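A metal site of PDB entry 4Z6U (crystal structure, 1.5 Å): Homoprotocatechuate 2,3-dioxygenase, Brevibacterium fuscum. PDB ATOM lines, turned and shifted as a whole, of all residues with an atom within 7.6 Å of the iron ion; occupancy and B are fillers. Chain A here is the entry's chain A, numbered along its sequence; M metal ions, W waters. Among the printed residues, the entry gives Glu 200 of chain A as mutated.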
ATOM      1  N   ASP A 154     -11.492   2.240  -4.556  1.00  0.00           N
ATOM      2  CA  ASP A 154     -10.721   1.723  -5.669  1.00  0.00           C
ATOM      3  C   ASP A 154      -9.225   2.076  -5.630  1.00  0.00           C
ATOM      4  O   ASP A 154      -8.371   1.212  -5.842  1.00  0.00           O
ATOM      5  CB  ASP A 154     -11.260   2.115  -7.041  1.00  0.00           C
ATOM      6  CG  ASP A 154     -10.559   1.327  -8.144  1.00  0.00           C
ATOM      7  OD1 ASP A 154     -10.792   0.085  -8.235  1.00  0.00           O
ATOM      8  OD2 ASP A 154      -9.721   1.937  -8.881  1.00  0.00           O
ATOM      9  N   HIS A 155      -8.925   3.343  -5.414  1.00  0.00           N
ATOM     10  CA  HIS A 155      -7.523   3.793  -5.509  1.00  0.00           C
ATOM     11  C   HIS A 155      -7.266   5.154  -4.921  1.00  0.00           C
ATOM     12  O   HIS A 155      -8.175   5.929  -4.623  1.00  0.00           O
ATOM     13  CB  HIS A 155      -7.021   3.776  -6.989  1.00  0.00           C
ATOM     14  CG  HIS A 155      -7.680   4.790  -7.881  1.00  0.00           C
ATOM     15  ND1 HIS A 155      -8.754   4.462  -8.675  1.00  0.00           N
ATOM     16  CD2 HIS A 155      -7.426   6.094  -8.107  1.00  0.00           C
ATOM     17  CE1 HIS A 155      -9.127   5.519  -9.368  1.00  0.00           C
ATOM     18  NE2 HIS A 155      -8.331   6.525  -9.047  1.00  0.00           N
ATOM     19  N   PHE A 156      -5.982   5.465  -4.822  1.00  0.00           N
ATOM     20  CA  PHE A 156      -5.510   6.791  -4.527  1.00  0.00           C
ATOM     21  C   PHE A 156      -4.763   7.346  -5.761  1.00  0.00           C
ATOM     22  O   PHE A 156      -4.293   6.573  -6.638  1.00  0.00           O
ATOM     23  CB  PHE A 156      -4.496   6.744  -3.363  1.00  0.00           C
ATOM     24  CG  PHE A 156      -4.926   5.959  -2.139  1.00  0.00           C
ATOM     25  CD1 PHE A 156      -6.090   6.279  -1.453  1.00  0.00           C
ATOM     26  CD2 PHE A 156      -4.153   4.894  -1.679  1.00  0.00           C
ATOM     27  CE1 PHE A 156      -6.453   5.569  -0.310  1.00  0.00           C
ATOM     28  CE2 PHE A 156      -4.531   4.179  -0.555  1.00  0.00           C
ATOM     29  CZ  PHE A 156      -5.684   4.520   0.128  1.00  0.00           C
ATOM     30  N   ASN A 157      -4.603   8.658  -5.819  1.00  0.00           N
ATOM     31  CA  ASN A 157      -3.736   9.268  -6.832  1.00  0.00           C
ATOM     32  C   ASN A 157      -2.923  10.367  -6.133  1.00  0.00           C
ATOM     33  O   ASN A 157      -3.470  11.223  -5.495  1.00  0.00           O
ATOM     34  CB  ASN A 157      -4.586   9.805  -7.989  1.00  0.00           C
ATOM     35  CG  ASN A 157      -3.764  10.299  -9.139  1.00  0.00           C
ATOM     36  OD1 ASN A 157      -2.938  11.167  -8.966  1.00  0.00           O
ATOM     37  ND2 ASN A 157      -3.976   9.735 -10.318  1.00  0.00           N
ATOM     38  N   TRP A 192       0.211   4.662 -13.571  1.00  0.00           N
ATOM     39  CA  TRP A 192      -0.775   3.954 -12.784  1.00  0.00           C
ATOM     40  C   TRP A 192      -0.228   2.612 -12.434  1.00  0.00           C
ATOM     41  O   TRP A 192       0.343   1.957 -13.293  1.00  0.00           O
ATOM     42  CB  TRP A 192      -2.043   3.806 -13.637  1.00  0.00           C
ATOM     43  CG  TRP A 192      -2.856   5.069 -13.801  1.00  0.00           C
ATOM     44  CD1 TRP A 192      -4.018   5.398 -13.135  1.00  0.00           C
ATOM     45  CD2 TRP A 192      -2.572   6.169 -14.653  1.00  0.00           C
ATOM     46  NE1 TRP A 192      -4.470   6.636 -13.519  1.00  0.00           N
ATOM     47  CE2 TRP A 192      -3.608   7.125 -14.472  1.00  0.00           C
ATOM     48  CE3 TRP A 192      -1.568   6.443 -15.609  1.00  0.00           C
ATOM     49  CZ2 TRP A 192      -3.650   8.329 -15.166  1.00  0.00           C
ATOM     50  CZ3 TRP A 192      -1.613   7.646 -16.294  1.00  0.00           C
ATOM     51  CH2 TRP A 192      -2.648   8.588 -16.069  1.00  0.00           C
ATOM     52  N   GLU A 200      -5.392   0.237 -11.000  1.00  0.00           N
ATOM     53  CA  GLU A 200      -4.645   0.990  -9.997  1.00  0.00           C
ATOM     54  C   GLU A 200      -5.088   0.693  -8.573  1.00  0.00           C
ATOM     55  O   GLU A 200      -6.278   0.530  -8.284  1.00  0.00           O
ATOM     56  CB  GLU A 200      -4.738   2.505 -10.285  1.00  0.00           C
ATOM     57  CG  GLU A 200      -6.170   2.931 -10.608  1.00  0.00           C
ATOM     58  CD  GLU A 200      -6.355   4.366 -11.096  1.00  0.00           C
ATOM     59  OE1 GLU A 200      -5.694   5.280 -10.550  1.00  0.00           O
ATOM     60  OE2 GLU A 200      -7.241   4.579 -12.009  1.00  0.00           O
ATOM     61  N   ALA A 203      -1.538   5.764  -7.995  1.00  0.00           N
ATOM     62  CA  ALA A 203      -1.161   6.366  -9.234  1.00  0.00           C
ATOM     63  C   ALA A 203      -0.362   7.619  -8.947  1.00  0.00           C
ATOM     64  O   ALA A 203      -0.520   8.247  -7.904  1.00  0.00           O
ATOM     65  CB  ALA A 203      -2.393   6.694 -10.076  1.00  0.00           C
ATOM     66  N   THR A 205       0.773  11.372 -10.504  1.00  0.00           N
ATOM     67  CA  THR A 205       0.516  12.484 -11.403  1.00  0.00           C
ATOM     68  C   THR A 205       1.659  13.463 -11.220  1.00  0.00           C
ATOM     69  O   THR A 205       1.934  13.904 -10.093  1.00  0.00           O
ATOM     70  CB  THR A 205      -0.820  13.159 -11.078  1.00  0.00           C
ATOM     71  OG1 THR A 205      -1.892  12.206 -11.190  1.00  0.00           O
ATOM     72  CG2 THR A 205      -1.091  14.336 -11.986  1.00  0.00           C
ATOM     73  N   HIS A 213      -3.797  13.909  -4.965  1.00  0.00           N
ATOM     74  CA  HIS A 213      -4.680  14.312  -6.020  1.00  0.00           C
ATOM     75  C   HIS A 213      -6.147  13.934  -5.758  1.00  0.00           C
ATOM     76  O   HIS A 213      -7.013  14.805  -5.819  1.00  0.00           O
ATOM     77  CB  HIS A 213      -4.221  13.795  -7.384  1.00  0.00           C
ATOM     78  CG  HIS A 213      -4.856  14.539  -8.500  1.00  0.00           C
ATOM     79  ND1 HIS A 213      -6.123  14.252  -8.946  1.00  0.00           N
ATOM     80  CD2 HIS A 213      -4.453  15.620  -9.208  1.00  0.00           C
ATOM     81  CE1 HIS A 213      -6.474  15.094  -9.901  1.00  0.00           C
ATOM     82  NE2 HIS A 213      -5.470  15.930 -10.094  1.00  0.00           N
ATOM     83  N   HIS A 214      -6.424  12.647  -5.497  1.00  0.00           N
ATOM     84  CA  HIS A 214      -7.766  12.236  -5.156  1.00  0.00           C
ATOM     85  C   HIS A 214      -7.780  10.861  -4.521  1.00  0.00           C
ATOM     86  O   HIS A 214      -6.797  10.158  -4.551  1.00  0.00           O
ATOM     87  CB  HIS A 214      -8.695  12.251  -6.406  1.00  0.00           C
ATOM     88  CG  HIS A 214      -8.264  11.338  -7.521  1.00  0.00           C
ATOM     89  ND1 HIS A 214      -7.539  11.786  -8.589  1.00  0.00           N
ATOM     90  CD2 HIS A 214      -8.482  10.020  -7.737  1.00  0.00           C
ATOM     91  CE1 HIS A 214      -7.319  10.796  -9.436  1.00  0.00           C
ATOM     92  NE2 HIS A 214      -7.881   9.709  -8.940  1.00  0.00           N
ATOM     93  N   VAL A 215      -8.968  10.535  -3.962  1.00  0.00           N
ATOM     94  CA  VAL A 215      -9.338   9.204  -3.528  1.00  0.00           C
ATOM     95  C   VAL A 215     -10.505   8.811  -4.419  1.00  0.00           C
ATOM     96  O   VAL A 215     -11.366   9.653  -4.693  1.00  0.00           O
ATOM     97  CB  VAL A 215      -9.754   9.209  -2.018  1.00  0.00           C
ATOM     98  CG1 VAL A 215     -10.175   7.836  -1.580  1.00  0.00           C
ATOM     99  CG2 VAL A 215      -8.567   9.715  -1.170  1.00  0.00           C
ATOM    100  N   ALA A 216     -10.521   7.553  -4.888  1.00  0.00           N
ATOM    101  CA  ALA A 216     -11.551   7.105  -5.809  1.00  0.00           C
ATOM    102  C   ALA A 216     -12.383   5.979  -5.213  1.00  0.00           C
ATOM    103  O   ALA A 216     -11.795   4.986  -4.699  1.00  0.00           O
ATOM    104  CB  ALA A 216     -10.917   6.607  -7.109  1.00  0.00           C
ATOM    105  N   HIS A 248     -12.606   7.577 -19.328  1.00  0.00           N
ATOM    106  CA  HIS A 248     -11.158   7.770 -19.377  1.00  0.00           C
ATOM    107  C   HIS A 248     -10.574   7.063 -20.604  1.00  0.00           C
ATOM    108  O   HIS A 248     -11.089   6.025 -21.029  1.00  0.00           O
ATOM    109  CB  HIS A 248     -10.527   7.124 -18.139  1.00  0.00           C
ATOM    110  CG  HIS A 248     -10.578   7.953 -16.896  1.00  0.00           C
ATOM    111  ND1 HIS A 248     -10.199   9.301 -16.866  1.00  0.00           N
ATOM    112  CD2 HIS A 248     -10.895   7.625 -15.627  1.00  0.00           C
ATOM    113  CE1 HIS A 248     -10.315   9.738 -15.627  1.00  0.00           C
ATOM    114  NE2 HIS A 248     -10.703   8.742 -14.856  1.00  0.00           N
ATOM    115  N   SER A 251      -7.111   3.714 -18.301  1.00  0.00           N
ATOM    116  CA  SER A 251      -7.966   2.905 -17.408  1.00  0.00           C
ATOM    117  C   SER A 251      -9.262   2.426 -18.071  1.00  0.00           C
ATOM    118  O   SER A 251      -9.823   1.459 -17.626  1.00  0.00           O
ATOM    119  CB  SER A 251      -8.304   3.564 -16.046  1.00  0.00           C
ATOM    120  OG  SER A 251      -9.398   4.438 -16.171  1.00  0.00           O
ATOM    121  N   TYR A 255     -16.069   7.850 -15.308  1.00  0.00           N
ATOM    122  CA  TYR A 255     -15.542   8.625 -14.185  1.00  0.00           C
ATOM    123  C   TYR A 255     -16.247   9.942 -13.955  1.00  0.00           C
ATOM    124  O   TYR A 255     -16.938  10.463 -14.836  1.00  0.00           O
ATOM    125  CB  TYR A 255     -14.029   8.910 -14.392  1.00  0.00           C
ATOM    126  CG  TYR A 255     -13.763   9.984 -15.424  1.00  0.00           C
ATOM    127  CD1 TYR A 255     -13.714  11.334 -15.061  1.00  0.00           C
ATOM    128  CD2 TYR A 255     -13.556   9.660 -16.773  1.00  0.00           C
ATOM    129  CE1 TYR A 255     -13.486  12.343 -15.973  1.00  0.00           C
ATOM    130  CE2 TYR A 255     -13.345  10.688 -17.713  1.00  0.00           C
ATOM    131  CZ  TYR A 255     -13.294  12.010 -17.308  1.00  0.00           C
ATOM    132  OH  TYR A 255     -13.055  12.976 -18.266  1.00  0.00           O
ATOM    133  N   TYR A 257     -15.222  13.588 -11.267  1.00  0.00           N
ATOM    134  CA  TYR A 257     -14.442  14.245 -10.182  1.00  0.00           C
ATOM    135  C   TYR A 257     -15.279  15.337  -9.541  1.00  0.00           C
ATOM    136  O   TYR A 257     -15.764  16.251 -10.218  1.00  0.00           O
ATOM    137  CB  TYR A 257     -13.165  14.857 -10.752  1.00  0.00           C
ATOM    138  CG  TYR A 257     -12.209  13.856 -11.334  1.00  0.00           C
ATOM    139  CD1 TYR A 257     -11.340  13.115 -10.530  1.00  0.00           C
ATOM    140  CD2 TYR A 257     -12.130  13.657 -12.707  1.00  0.00           C
ATOM    141  CE1 TYR A 257     -10.440  12.200 -11.062  1.00  0.00           C
ATOM    142  CE2 TYR A 257     -11.226  12.729 -13.250  1.00  0.00           C
ATOM    143  CZ  TYR A 257     -10.381  12.010 -12.443  1.00  0.00           C
ATOM    144  OH  TYR A 257      -9.492  11.133 -12.997  1.00  0.00           O
ATOM    145  N   GLU A 267     -12.861  11.003  -6.783  1.00  0.00           N
ATOM    146  CA  GLU A 267     -13.275  10.431  -8.049  1.00  0.00           C
ATOM    147  C   GLU A 267     -14.309   9.340  -7.814  1.00  0.00           C
ATOM    148  O   GLU A 267     -14.158   8.519  -6.896  1.00  0.00           O
ATOM    149  CB  GLU A 267     -12.079   9.804  -8.782  1.00  0.00           C
ATOM    150  CG  GLU A 267     -12.410   9.394 -10.200  1.00  0.00           C
ATOM    151  CD  GLU A 267     -11.274   8.768 -10.939  1.00  0.00           C
ATOM    152  OE1 GLU A 267     -10.246   8.439 -10.296  1.00  0.00           O
ATOM    153  OE2 GLU A 267     -11.386   8.646 -12.181  1.00  0.00           O
ATOM    154  N   ILE A 268     -15.308   9.320  -8.689  1.00  0.00           N
ATOM    155  CA  ILE A 268     -16.182   8.164  -8.787  1.00  0.00           C
ATOM    156  C   ILE A 268     -15.912   7.472 -10.108  1.00  0.00           C
ATOM    157  O   ILE A 268     -15.744   8.132 -11.128  1.00  0.00           O
ATOM    158  CB  ILE A 268     -17.666   8.580  -8.701  1.00  0.00           C
ATOM    159  CG1 ILE A 268     -17.920   9.752  -7.724  1.00  0.00           C
ATOM    160  CG2 ILE A 268     -18.515   7.361  -8.382  1.00  0.00           C
ATOM    161  CD1 ILE A 268     -17.630   9.433  -6.296  1.00  0.00           C
ATOM    162  N   TYR A 269     -15.833   6.160 -10.058  1.00  0.00           N
ATOM    163  CA  TYR A 269     -15.105   5.338 -11.074  1.00  0.00           C
ATOM    164  C   TYR A 269     -15.858   4.034 -11.301  1.00  0.00           C
ATOM    165  O   TYR A 269     -16.364   3.434 -10.336  1.00  0.00           O
ATOM    166  CB  TYR A 269     -13.730   5.100 -10.487  1.00  0.00           C
ATOM    167  CG  TYR A 269     -12.648   4.430 -11.269  1.00  0.00           C
ATOM    168  CD1 TYR A 269     -11.738   5.176 -12.021  1.00  0.00           C
ATOM    169  CD2 TYR A 269     -12.425   3.048 -11.136  1.00  0.00           C
ATOM    170  CE1 TYR A 269     -10.645   4.577 -12.632  1.00  0.00           C
ATOM    171  CE2 TYR A 269     -11.358   2.422 -11.763  1.00  0.00           C
ATOM    172  CZ  TYR A 269     -10.463   3.188 -12.497  1.00  0.00           C
ATOM    173  OH  TYR A 269      -9.400   2.571 -13.080  1.00  0.00           O
ATOM    174  N   ARG A 293      -7.080  11.225 -21.521  1.00  0.00           N
ATOM    175  CA  ARG A 293      -7.641  11.442 -20.200  1.00  0.00           C
ATOM    176  C   ARG A 293      -9.158  11.367 -20.236  1.00  0.00           C
ATOM    177  O   ARG A 293      -9.775  10.701 -19.411  1.00  0.00           O
ATOM    178  CB  ARG A 293      -7.171  12.776 -19.636  1.00  0.00           C
ATOM    179  CG  ARG A 293      -5.717  12.736 -19.154  1.00  0.00           C
ATOM    180  CD  ARG A 293      -5.377  13.758 -18.111  1.00  0.00           C
ATOM    181  NE  ARG A 293      -4.018  13.556 -17.583  1.00  0.00           N
ATOM    182  CZ  ARG A 293      -3.637  12.751 -16.586  1.00  0.00           C
ATOM    183  NH1 ARG A 293      -4.513  11.976 -15.944  1.00  0.00           N
ATOM    184  NH2 ARG A 293      -2.356  12.716 -16.186  1.00  0.00           N
ATOM    185  N   TRP A 304      -7.861  20.789 -12.449  1.00  0.00           N
ATOM    186  CA  TRP A 304      -7.553  19.372 -12.268  1.00  0.00           C
ATOM    187  C   TRP A 304      -6.039  19.130 -12.207  1.00  0.00           C
ATOM    188  O   TRP A 304      -5.543  18.210 -11.537  1.00  0.00           O
ATOM    189  CB  TRP A 304      -8.257  18.550 -13.404  1.00  0.00           C
ATOM    190  CG  TRP A 304      -8.342  17.133 -13.089  1.00  0.00           C
ATOM    191  CD1 TRP A 304      -9.367  16.506 -12.422  1.00  0.00           C
ATOM    192  CD2 TRP A 304      -7.378  16.123 -13.390  1.00  0.00           C
ATOM    193  NE1 TRP A 304      -9.071  15.178 -12.270  1.00  0.00           N
ATOM    194  CE2 TRP A 304      -7.871  14.912 -12.876  1.00  0.00           C
ATOM    195  CE3 TRP A 304      -6.117  16.125 -14.034  1.00  0.00           C
ATOM    196  CZ2 TRP A 304      -7.150  13.722 -12.937  1.00  0.00           C
ATOM    197  CZ3 TRP A 304      -5.422  14.966 -14.103  1.00  0.00           C
ATOM    198  CH2 TRP A 304      -5.938  13.762 -13.589  1.00  0.00           C
HETATM  199 FE    FE M   1      -8.162   8.194 -10.530  1.00  0.00          FE
HETATM  200  O   HOH W   1      -7.979   9.569 -12.155  1.00  0.00           O
HETATM  201  O   HOH W   2      -8.459   7.005 -12.153  1.00  0.00           O
HETATM  202  O   HOH W   3      -6.019   7.841 -10.805  1.00  0.00           O
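The side-chain carboxylate (OE2) of Glu 267 sits at hydrogen-bond distance from a ring nitrogen (NE2) of His 248.
The side-chain carboxylate of Glu 200 sits at hydrogen-bond distance from the side-chain hydroxyl of Tyr 269 (3.1 Å).
The backbone carbonyl oxygen (O) of His 214 lies within hydrogen-bond range of the backbone NH (N) of Asn 157 (2.9 Å).
A ring nitrogen (ND1) of His 213 is in hydrogen-bond range of a ring nitrogen (ND1) of His 214, at 2.9 Å.
The side-chain carboxylate (OE1) of Glu 200 sits close to the indole nitrogen (NE1) of Trp 192.
The side-chain carboxylate (OE2) of Glu 267 sits at hydrogen-bond distance from the side-chain hydroxyl (OH) of Tyr 257, 3.2 Å away.
A ring nitrogen (NE2) of His 155 lies close to the side-chain carboxylate (OE1) of Glu 200, at 3.3 Å.
The backbone carbonyl oxygen of His 155 lies within hydrogen-bond range of the backbone NH of Ala 216 (2.9 Å).
OE1 of Glu 200 touches the iron ion, 3.8 Å away.
The nearest printed residue that does not touch the iron ion is Tyr 257 (4.1 Å).
The iron ion is bound by water W2 (2.0 Å), the side-chain carboxylate of Glu 267 (2.1 Å), water W1 (2.1 Å), water W3 (2.2 Å), a ring nitrogen (NE2) of His 214 (2.2 Å) and a ring nitrogen (NE2) of His 155 (2.2 Å).
The iron ion has six donor atoms within binding distance.
Water W3 lies within hydrogen-bond range of OE1 of Glu 200, ND2 of Asn 157 and NE1 of Trp 192.
Water W2 lies within hydrogen-bond range of OE2 of Glu 200 (2.7 Å) and OE2 of Glu 267 (3.4 Å).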
